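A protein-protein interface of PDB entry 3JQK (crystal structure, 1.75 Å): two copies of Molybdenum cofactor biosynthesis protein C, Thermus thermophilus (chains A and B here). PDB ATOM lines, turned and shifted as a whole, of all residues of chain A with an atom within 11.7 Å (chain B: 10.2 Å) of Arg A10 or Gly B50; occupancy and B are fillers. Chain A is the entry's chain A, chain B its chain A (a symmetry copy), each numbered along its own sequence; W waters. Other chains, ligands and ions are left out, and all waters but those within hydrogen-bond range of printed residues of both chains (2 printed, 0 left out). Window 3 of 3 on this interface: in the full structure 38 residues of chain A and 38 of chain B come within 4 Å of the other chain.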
ATOM      1  N   ARG A  10     -36.325  -4.052 -23.767  1.00  0.00           N
ATOM      2  CA  ARG A  10     -36.696  -2.996 -22.782  1.00  0.00           C
ATOM      3  C   ARG A  10     -35.974  -3.239 -21.457  1.00  0.00           C
ATOM      4  O   ARG A  10     -35.497  -4.345 -21.196  1.00  0.00           O
ATOM      5  CB  ARG A  10     -38.212  -3.005 -22.556  1.00  0.00           C
ATOM      6  CG  ARG A  10     -38.725  -4.221 -21.798  1.00  0.00           C
ATOM      7  CD  ARG A  10     -40.248  -4.218 -21.704  1.00  0.00           C
ATOM      8  NE  ARG A  10     -40.875  -4.815 -22.880  1.00  0.00           N
ATOM      9  CZ  ARG A  10     -40.916  -6.123 -23.122  1.00  0.00           C
ATOM     10  NH1 ARG A  10     -40.368  -6.976 -22.267  1.00  0.00           N
ATOM     11  NH2 ARG A  10     -41.501  -6.580 -24.220  1.00  0.00           N
ATOM     12  N   PRO A  11     -35.871  -2.203 -20.606  1.00  0.00           N
ATOM     13  CA  PRO A  11     -35.198  -2.347 -19.311  1.00  0.00           C
ATOM     14  C   PRO A  11     -35.910  -3.357 -18.415  1.00  0.00           C
ATOM     15  O   PRO A  11     -37.134  -3.480 -18.461  1.00  0.00           O
ATOM     16  CB  PRO A  11     -35.271  -0.938 -18.723  1.00  0.00           C
ATOM     17  CG  PRO A  11     -35.271  -0.057 -19.944  1.00  0.00           C
ATOM     18  CD  PRO A  11     -36.217  -0.793 -20.865  1.00  0.00           C
ATOM     19  N   ARG A  12     -35.147  -4.080 -17.601  1.00  0.00           N
ATOM     20  CA  ARG A  12     -35.747  -5.042 -16.687  1.00  0.00           C
ATOM     21  C   ARG A  12     -34.784  -5.489 -15.598  1.00  0.00           C
ATOM     22  O   ARG A  12     -33.569  -5.506 -15.794  1.00  0.00           O
ATOM     23  CB  ARG A  12     -36.251  -6.277 -17.444  1.00  0.00           C
ATOM     24  CG  ARG A  12     -35.164  -7.248 -17.895  1.00  0.00           C
ATOM     25  CD  ARG A  12     -35.764  -8.626 -18.158  1.00  0.00           C
ATOM     26  NE  ARG A  12     -34.756  -9.650 -18.424  1.00  0.00           N
ATOM     27  CZ  ARG A  12     -34.056  -9.739 -19.550  1.00  0.00           C
ATOM     28  NH1 ARG A  12     -34.252  -8.866 -20.529  1.00  0.00           N
ATOM     29  NH2 ARG A  12     -33.161 -10.707 -19.700  1.00  0.00           N
ATOM     30  N   MET A  13     -35.331  -5.828 -14.437  1.00  0.00           N
ATOM     31  CA  MET A  13     -34.509  -6.318 -13.343  1.00  0.00           C
ATOM     32  C   MET A  13     -34.440  -7.813 -13.626  1.00  0.00           C
ATOM     33  O   MET A  13     -35.406  -8.543 -13.395  1.00  0.00           O
ATOM     34  CB  MET A  13     -35.167  -6.056 -11.988  1.00  0.00           C
ATOM     35  CG  MET A  13     -34.300  -6.469 -10.816  1.00  0.00           C
ATOM     36  SD  MET A  13     -35.169  -6.499  -9.246  1.00  0.00           S
ATOM     37  CE  MET A  13     -35.324  -4.759  -8.932  1.00  0.00           C
ATOM     38  N   VAL A  14     -33.299  -8.247 -14.152  1.00  0.00           N
ATOM     39  CA  VAL A  14     -33.076  -9.645 -14.502  1.00  0.00           C
ATOM     40  C   VAL A  14     -33.521 -10.650 -13.447  1.00  0.00           C
ATOM     41  O   VAL A  14     -33.162 -10.545 -12.274  1.00  0.00           O
ATOM     42  CB  VAL A  14     -31.578  -9.910 -14.752  1.00  0.00           C
ATOM     43  CG1 VAL A  14     -31.370 -11.355 -15.179  1.00  0.00           C
ATOM     44  CG2 VAL A  14     -31.058  -8.960 -15.817  1.00  0.00           C
ATOM     45  N   ASP A  15     -34.307 -11.629 -13.885  1.00  0.00           N
ATOM     46  CA  ASP A  15     -34.822 -12.665 -13.004  1.00  0.00           C
ATOM     47  C   ASP A  15     -33.725 -13.614 -12.528  1.00  0.00           C
ATOM     48  O   ASP A  15     -33.082 -14.289 -13.333  1.00  0.00           O
ATOM     49  CB  ASP A  15     -35.916 -13.447 -13.739  1.00  0.00           C
ATOM     50  CG  ASP A  15     -36.651 -14.419 -12.838  1.00  0.00           C
ATOM     51  OD1 ASP A  15     -37.529 -15.149 -13.345  1.00  0.00           O
ATOM     52  OD2 ASP A  15     -36.359 -14.455 -11.624  1.00  0.00           O
ATOM     53  N   PRO A  72     -31.579   2.151 -11.049  1.00  0.00           N
ATOM     54  CA  PRO A  72     -32.844   1.604 -11.557  1.00  0.00           C
ATOM     55  C   PRO A  72     -33.054   0.093 -11.619  1.00  0.00           C
ATOM     56  O   PRO A  72     -34.010  -0.418 -11.041  1.00  0.00           O
ATOM     57  CB  PRO A  72     -32.977   2.261 -12.928  1.00  0.00           C
ATOM     58  CG  PRO A  72     -32.369   3.609 -12.693  1.00  0.00           C
ATOM     59  CD  PRO A  72     -31.110   3.250 -11.917  1.00  0.00           C
ATOM     60  N   LEU A  73     -32.172  -0.624 -12.306  1.00  0.00           N
ATOM     61  CA  LEU A  73     -32.337  -2.068 -12.443  1.00  0.00           C
ATOM     62  C   LEU A  73     -31.612  -2.919 -11.406  1.00  0.00           C
ATOM     63  O   LEU A  73     -31.556  -4.144 -11.527  1.00  0.00           O
ATOM     64  CB  LEU A  73     -31.904  -2.496 -13.846  1.00  0.00           C
ATOM     65  CG  LEU A  73     -32.545  -1.696 -14.980  1.00  0.00           C
ATOM     66  CD1 LEU A  73     -31.991  -2.179 -16.323  1.00  0.00           C
ATOM     67  CD2 LEU A  73     -34.067  -1.847 -14.920  1.00  0.00           C
ATOM     68  N   CYS A  74     -31.077  -2.273 -10.379  1.00  0.00           N
ATOM     69  CA  CYS A  74     -30.345  -2.969  -9.327  1.00  0.00           C
ATOM     70  C   CYS A  74     -31.265  -3.773  -8.409  1.00  0.00           C
ATOM     71  O   CYS A  74     -32.328  -3.296  -8.006  1.00  0.00           O
ATOM     72  CB  CYS A  74     -29.545  -1.952  -8.510  1.00  0.00           C
ATOM     73  SG  CYS A  74     -28.571  -2.652  -7.171  1.00  0.00           S
ATOM     74  N   ALA B  38     -17.489  -3.196 -24.436  1.00  0.00           N
ATOM     75  CA  ALA B  38     -18.565  -2.335 -23.945  1.00  0.00           C
ATOM     76  C   ALA B  38     -19.118  -1.439 -25.059  1.00  0.00           C
ATOM     77  O   ALA B  38     -20.331  -1.226 -25.155  1.00  0.00           O
ATOM     78  CB  ALA B  38     -18.064  -1.477 -22.787  1.00  0.00           C
ATOM     79  N   ALA B  41     -21.456  -3.404 -27.292  1.00  0.00           N
ATOM     80  CA  ALA B  41     -22.720  -3.584 -26.586  1.00  0.00           C
ATOM     81  C   ALA B  41     -23.583  -2.328 -26.649  1.00  0.00           C
ATOM     82  O   ALA B  41     -24.768  -2.397 -26.972  1.00  0.00           O
ATOM     83  CB  ALA B  41     -22.455  -3.963 -25.132  1.00  0.00           C
ATOM     84  N   LEU B  42     -22.991  -1.179 -26.338  1.00  0.00           N
ATOM     85  CA  LEU B  42     -23.727   0.080 -26.363  1.00  0.00           C
ATOM     86  C   LEU B  42     -24.263   0.408 -27.750  1.00  0.00           C
ATOM     87  O   LEU B  42     -25.284   1.083 -27.882  1.00  0.00           O
ATOM     88  CB  LEU B  42     -22.846   1.234 -25.876  1.00  0.00           C
ATOM     89  CG  LEU B  42     -22.680   1.387 -24.363  1.00  0.00           C
ATOM     90  CD1 LEU B  42     -21.719   2.527 -24.064  1.00  0.00           C
ATOM     91  CD2 LEU B  42     -24.039   1.654 -23.726  1.00  0.00           C
ATOM     92  N   GLU B  43     -23.574  -0.065 -28.782  1.00  0.00           N
ATOM     93  CA  GLU B  43     -24.006   0.191 -30.148  1.00  0.00           C
ATOM     94  C   GLU B  43     -25.167  -0.729 -30.513  1.00  0.00           C
ATOM     95  O   GLU B  43     -25.991  -0.398 -31.365  1.00  0.00           O
ATOM     96  CB  GLU B  43     -22.833   0.011 -31.115  1.00  0.00           C
ATOM     97  CG  GLU B  43     -21.677   0.964 -30.826  1.00  0.00           C
ATOM     98  CD  GLU B  43     -20.536   0.837 -31.816  1.00  0.00           C
ATOM     99  OE1 GLU B  43     -20.080  -0.299 -32.058  1.00  0.00           O
ATOM    100  OE2 GLU B  43     -20.087   1.877 -32.342  1.00  0.00           O
ATOM    101  N   LYS B  44     -25.231  -1.886 -29.860  1.00  0.00           N
ATOM    102  CA  LYS B  44     -26.313  -2.835 -30.096  1.00  0.00           C
ATOM    103  C   LYS B  44     -27.529  -2.397 -29.284  1.00  0.00           C
ATOM    104  O   LYS B  44     -28.647  -2.857 -29.518  1.00  0.00           O
ATOM    105  CB  LYS B  44     -25.898  -4.247 -29.667  1.00  0.00           C
ATOM    106  CG  LYS B  44     -25.095  -5.021 -30.702  1.00  0.00           C
ATOM    107  CD  LYS B  44     -23.789  -4.335 -31.049  1.00  0.00           C
ATOM    108  CE  LYS B  44     -22.955  -5.192 -31.984  1.00  0.00           C
ATOM    109  NZ  LYS B  44     -21.606  -4.607 -32.210  1.00  0.00           N
ATOM    110  N   GLY B  45     -27.299  -1.499 -28.332  1.00  0.00           N
ATOM    111  CA  GLY B  45     -28.377  -1.013 -27.492  1.00  0.00           C
ATOM    112  C   GLY B  45     -28.332  -1.631 -26.109  1.00  0.00           C
ATOM    113  O   GLY B  45     -29.365  -1.814 -25.465  1.00  0.00           O
ATOM    114  N   LYS B  49     -30.976  -6.151 -21.438  1.00  0.00           N
ATOM    115  CA  LYS B  49     -31.296  -5.550 -20.147  1.00  0.00           C
ATOM    116  C   LYS B  49     -31.819  -4.130 -20.328  1.00  0.00           C
ATOM    117  O   LYS B  49     -32.318  -3.523 -19.382  1.00  0.00           O
ATOM    118  CB  LYS B  49     -30.055  -5.528 -19.249  1.00  0.00           C
ATOM    119  CG  LYS B  49     -30.291  -4.954 -17.853  1.00  0.00           C
ATOM    120  CD  LYS B  49     -29.010  -4.918 -17.023  1.00  0.00           C
ATOM    121  CE  LYS B  49     -29.285  -4.397 -15.617  1.00  0.00           C
ATOM    122  NZ  LYS B  49     -28.063  -4.350 -14.769  1.00  0.00           N
ATOM    123  N   GLY B  50     -31.700  -3.606 -21.545  1.00  0.00           N
ATOM    124  CA  GLY B  50     -32.161  -2.256 -21.823  1.00  0.00           C
ATOM    125  C   GLY B  50     -31.044  -1.352 -22.312  1.00  0.00           C
ATOM    126  O   GLY B  50     -29.870  -1.712 -22.234  1.00  0.00           O
ATOM    127  N   ASP B  51     -31.411  -0.176 -22.816  1.00  0.00           N
ATOM    128  CA  ASP B  51     -30.448   0.800 -23.326  1.00  0.00           C
ATOM    129  C   ASP B  51     -29.767   1.520 -22.159  1.00  0.00           C
ATOM    130  O   ASP B  51     -30.396   2.311 -21.457  1.00  0.00           O
ATOM    131  CB  ASP B  51     -31.167   1.831 -24.199  1.00  0.00           C
ATOM    132  CG  ASP B  51     -30.209   2.703 -24.990  1.00  0.00           C
ATOM    133  OD1 ASP B  51     -29.144   3.074 -24.453  1.00  0.00           O
ATOM    134  OD2 ASP B  51     -30.534   3.029 -26.152  1.00  0.00           O
ATOM    135  N   PRO B  52     -28.468   1.262 -21.945  1.00  0.00           N
ATOM    136  CA  PRO B  52     -27.734   1.903 -20.848  1.00  0.00           C
ATOM    137  C   PRO B  52     -27.833   3.429 -20.807  1.00  0.00           C
ATOM    138  O   PRO B  52     -27.983   4.020 -19.739  1.00  0.00           O
ATOM    139  CB  PRO B  52     -26.297   1.432 -21.073  1.00  0.00           C
ATOM    140  CG  PRO B  52     -26.485   0.080 -21.700  1.00  0.00           C
ATOM    141  CD  PRO B  52     -27.594   0.339 -22.690  1.00  0.00           C
ATOM    142  N   LEU B  53     -27.753   4.065 -21.969  1.00  0.00           N
ATOM    143  CA  LEU B  53     -27.805   5.520 -22.033  1.00  0.00           C
ATOM    144  C   LEU B  53     -29.153   6.099 -21.619  1.00  0.00           C
ATOM    145  O   LEU B  53     -29.214   7.147 -20.976  1.00  0.00           O
ATOM    146  CB  LEU B  53     -27.443   5.990 -23.443  1.00  0.00           C
ATOM    147  CG  LEU B  53     -26.169   5.373 -24.029  1.00  0.00           C
ATOM    148  CD1 LEU B  53     -25.822   6.072 -25.331  1.00  0.00           C
ATOM    149  CD2 LEU B  53     -25.022   5.504 -23.041  1.00  0.00           C
ATOM    150  N   VAL B  54     -30.232   5.415 -21.980  1.00  0.00           N
ATOM    151  CA  VAL B  54     -31.571   5.883 -21.643  1.00  0.00           C
ATOM    152  C   VAL B  54     -31.863   5.729 -20.150  1.00  0.00           C
ATOM    153  O   VAL B  54     -32.365   6.650 -19.504  1.00  0.00           O
ATOM    154  CB  VAL B  54     -32.643   5.114 -22.443  1.00  0.00           C
ATOM    155  CG1 VAL B  54     -34.031   5.572 -22.024  1.00  0.00           C
ATOM    156  CG2 VAL B  54     -32.440   5.341 -23.939  1.00  0.00           C
ATOM    157  N   VAL B  55     -31.550   4.563 -19.604  1.00  0.00           N
ATOM    158  CA  VAL B  55     -31.791   4.312 -18.188  1.00  0.00           C
ATOM    159  C   VAL B  55     -30.933   5.233 -17.318  1.00  0.00           C
ATOM    160  O   VAL B  55     -31.399   5.768 -16.315  1.00  0.00           O
ATOM    161  CB  VAL B  55     -31.502   2.827 -17.847  1.00  0.00           C
ATOM    162  CG1 VAL B  55     -31.720   2.566 -16.354  1.00  0.00           C
ATOM    163  CG2 VAL B  55     -32.418   1.928 -18.675  1.00  0.00           C
ATOM    164  N   ALA B  56     -29.680   5.433 -17.720  1.00  0.00           N
ATOM    165  CA  ALA B  56     -28.760   6.280 -16.965  1.00  0.00           C
ATOM    166  C   ALA B  56     -29.203   7.737 -16.924  1.00  0.00           C
ATOM    167  O   ALA B  56     -29.054   8.418 -15.908  1.00  0.00           O
ATOM    168  CB  ALA B  56     -27.349   6.177 -17.566  1.00  0.00           C
ATOM    169  N   THR B 123     -24.945   4.140 -13.296  1.00  0.00           N
ATOM    170  CA  THR B 123     -25.973   3.366 -13.979  1.00  0.00           C
ATOM    171  C   THR B 123     -25.458   2.810 -15.301  1.00  0.00           C
ATOM    172  O   THR B 123     -25.766   1.675 -15.667  1.00  0.00           O
ATOM    173  CB  THR B 123     -27.238   4.209 -14.187  1.00  0.00           C
ATOM    174  OG1 THR B 123     -27.754   4.574 -12.903  1.00  0.00           O
ATOM    175  CG2 THR B 123     -28.302   3.416 -14.940  1.00  0.00           C
ATOM    176  N   VAL B 124     -24.667   3.601 -16.016  1.00  0.00           N
ATOM    177  CA  VAL B 124     -24.085   3.125 -17.263  1.00  0.00           C
ATOM    178  C   VAL B 124     -23.219   1.915 -16.904  1.00  0.00           C
ATOM    179  O   VAL B 124     -23.249   0.890 -17.585  1.00  0.00           O
ATOM    180  CB  VAL B 124     -23.195   4.202 -17.921  1.00  0.00           C
ATOM    181  CG1 VAL B 124     -22.376   3.585 -19.062  1.00  0.00           C
ATOM    182  CG2 VAL B 124     -24.060   5.332 -18.453  1.00  0.00           C
ATOM    183  N   ASP B 126     -23.544  -0.072 -14.338  1.00  0.00           N
ATOM    184  CA  ASP B 126     -24.411  -1.189 -13.974  1.00  0.00           C
ATOM    185  C   ASP B 126     -24.912  -1.955 -15.194  1.00  0.00           C
ATOM    186  O   ASP B 126     -24.965  -3.189 -15.181  1.00  0.00           O
ATOM    187  CB  ASP B 126     -25.622  -0.697 -13.172  1.00  0.00           C
ATOM    188  CG  ASP B 126     -26.571  -1.830 -12.805  1.00  0.00           C
ATOM    189  OD1 ASP B 126     -26.116  -2.780 -12.143  1.00  0.00           O
ATOM    190  OD2 ASP B 126     -27.764  -1.771 -13.178  1.00  0.00           O
ATOM    191  N   MET B 127     -25.261  -1.214 -16.242  1.00  0.00           N
ATOM    192  CA  MET B 127     -25.800  -1.784 -17.478  1.00  0.00           C
ATOM    193  C   MET B 127     -24.758  -2.460 -18.369  1.00  0.00           C
ATOM    194  O   MET B 127     -25.119  -3.191 -19.291  1.00  0.00           O
ATOM    195  CB  MET B 127     -26.479  -0.695 -18.320  1.00  0.00           C
ATOM    196  CG  MET B 127     -27.344   0.325 -17.585  1.00  0.00           C
ATOM    197  SD  MET B 127     -29.092  -0.092 -17.402  1.00  0.00           S
ATOM    198  CE  MET B 127     -29.554  -0.536 -19.071  1.00  0.00           C
ATOM    199  N   LEU B 128     -23.477  -2.217 -18.113  1.00  0.00           N
ATOM    200  CA  LEU B 128     -22.424  -2.796 -18.950  1.00  0.00           C
ATOM    201  C   LEU B 128     -21.384  -3.643 -18.223  1.00  0.00           C
ATOM    202  O   LEU B 128     -20.500  -4.219 -18.862  1.00  0.00           O
ATOM    203  CB  LEU B 128     -21.696  -1.680 -19.708  1.00  0.00           C
ATOM    204  CG  LEU B 128     -22.499  -0.772 -20.640  1.00  0.00           C
ATOM    205  CD1 LEU B 128     -21.596   0.348 -21.153  1.00  0.00           C
ATOM    206  CD2 LEU B 128     -23.065  -1.582 -21.803  1.00  0.00           C
ATOM    207  N   LYS B 129     -21.482  -3.731 -16.901  1.00  0.00           N
ATOM    208  CA  LYS B 129     -20.509  -4.493 -16.122  1.00  0.00           C
ATOM    209  C   LYS B 129     -20.554  -6.007 -16.337  1.00  0.00           C
ATOM    210  O   LYS B 129     -19.579  -6.707 -16.053  1.00  0.00           O
ATOM    211  CB  LYS B 129     -20.675  -4.194 -14.631  1.00  0.00           C
ATOM    212  CG  LYS B 129     -21.931  -4.776 -14.001  1.00  0.00           C
ATOM    213  CD  LYS B 129     -21.981  -4.452 -12.518  1.00  0.00           C
ATOM    214  CE  LYS B 129     -23.065  -5.247 -11.815  1.00  0.00           C
ATOM    215  NZ  LYS B 129     -24.386  -5.059 -12.468  1.00  0.00           N
HETATM  216  O   HOH W   1     -33.474  -6.313 -22.940  1.00  0.00           O
HETATM  217  O   HOH W   2     -29.700   0.139 -13.820  1.00  0.00           O
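Arg A10 touches just these residues of chain B: Lys B49 and Gly B50. Pro A11 touches three residues of chain B. Asp A15 touches none of the printed residues of chain B. Printed residues of chain B within 4 Å of Pro A72: Val B55 and Thr B123. Printed residues of chain B within 4 Å of Leu A73: Lys B49 (3.4 Å) and Met B127 (3.7 Å). Lys B44 touches none of the printed residues of chain A. No residue of chain A comes within 4 Å of Pro B52. The nearest residue of chain B that does not touch Arg A10 is Asp B51 (5.7 Å). The nearest printed residue of chain B that does not touch Leu A73 is Asp B126 (4.3 Å).
Of the 9 printed residues of chain A, 5 touch a printed residue of chain B. Printed residues of chain A that touch a printed residue of chain B: Arg A10, Pro A11, Arg A12, Pro A72 and Leu A73. Hydrophobic or aromatic side chains of chain A that line the printed part of chain B: Pro A11, Pro A72 and Leu A73. Among the printed residues, 10 pairs touch across the chains. Among the printed residues, no Asp or Glu carboxylate lies within 4 Å of a Lys or Arg side-chain nitrogen of the other chain.
The side-chain amino group of Lys B49 is in salt-bridge range of the side-chain carboxylate of Asp B126 (3.0 Å).
Water W2 lies within hydrogen-bond range of the side-chain carboxylate (OD2) of Asp B126 (2.8 Å), the backbone NH (N) of Leu A73 (3.0 Å) and the side-chain sulfur (SD) of Met B127 (3.6 Å). Water W1 lies within hydrogen-bond range of the backbone NH (N) of Lys B49 (2.9 Å) and the backbone carbonyl oxygen (O) of Arg A10 (3.3 Å).
No position is printed for both chains.
N of Arg A12 lies within hydrogen-bond range of O of Lys B49 (3.4 Å).
O of Arg A10 touches O of Lys B49, at 3.8 Å. O of Arg A10 touches N of Gly B50 (3.9 Å). CA of Pro A11 touches O of Lys B49, at 3.1 Å. N of Pro A11 touches CA of Gly B50, at 3.9 Å. Pro A11 touches Val B55 (CG to CG2, 3.7 Å). CB of Pro A72 touches CG1 of Val B55, 3.7 Å away. OG1 of Thr B123 touches CD of Pro A72, at 3.7 Å. Lys B49 touches Leu A73 (O to CD1, 3.4 Å). Met B127 touches Leu A73 (SD to CD1, 3.7 Å).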
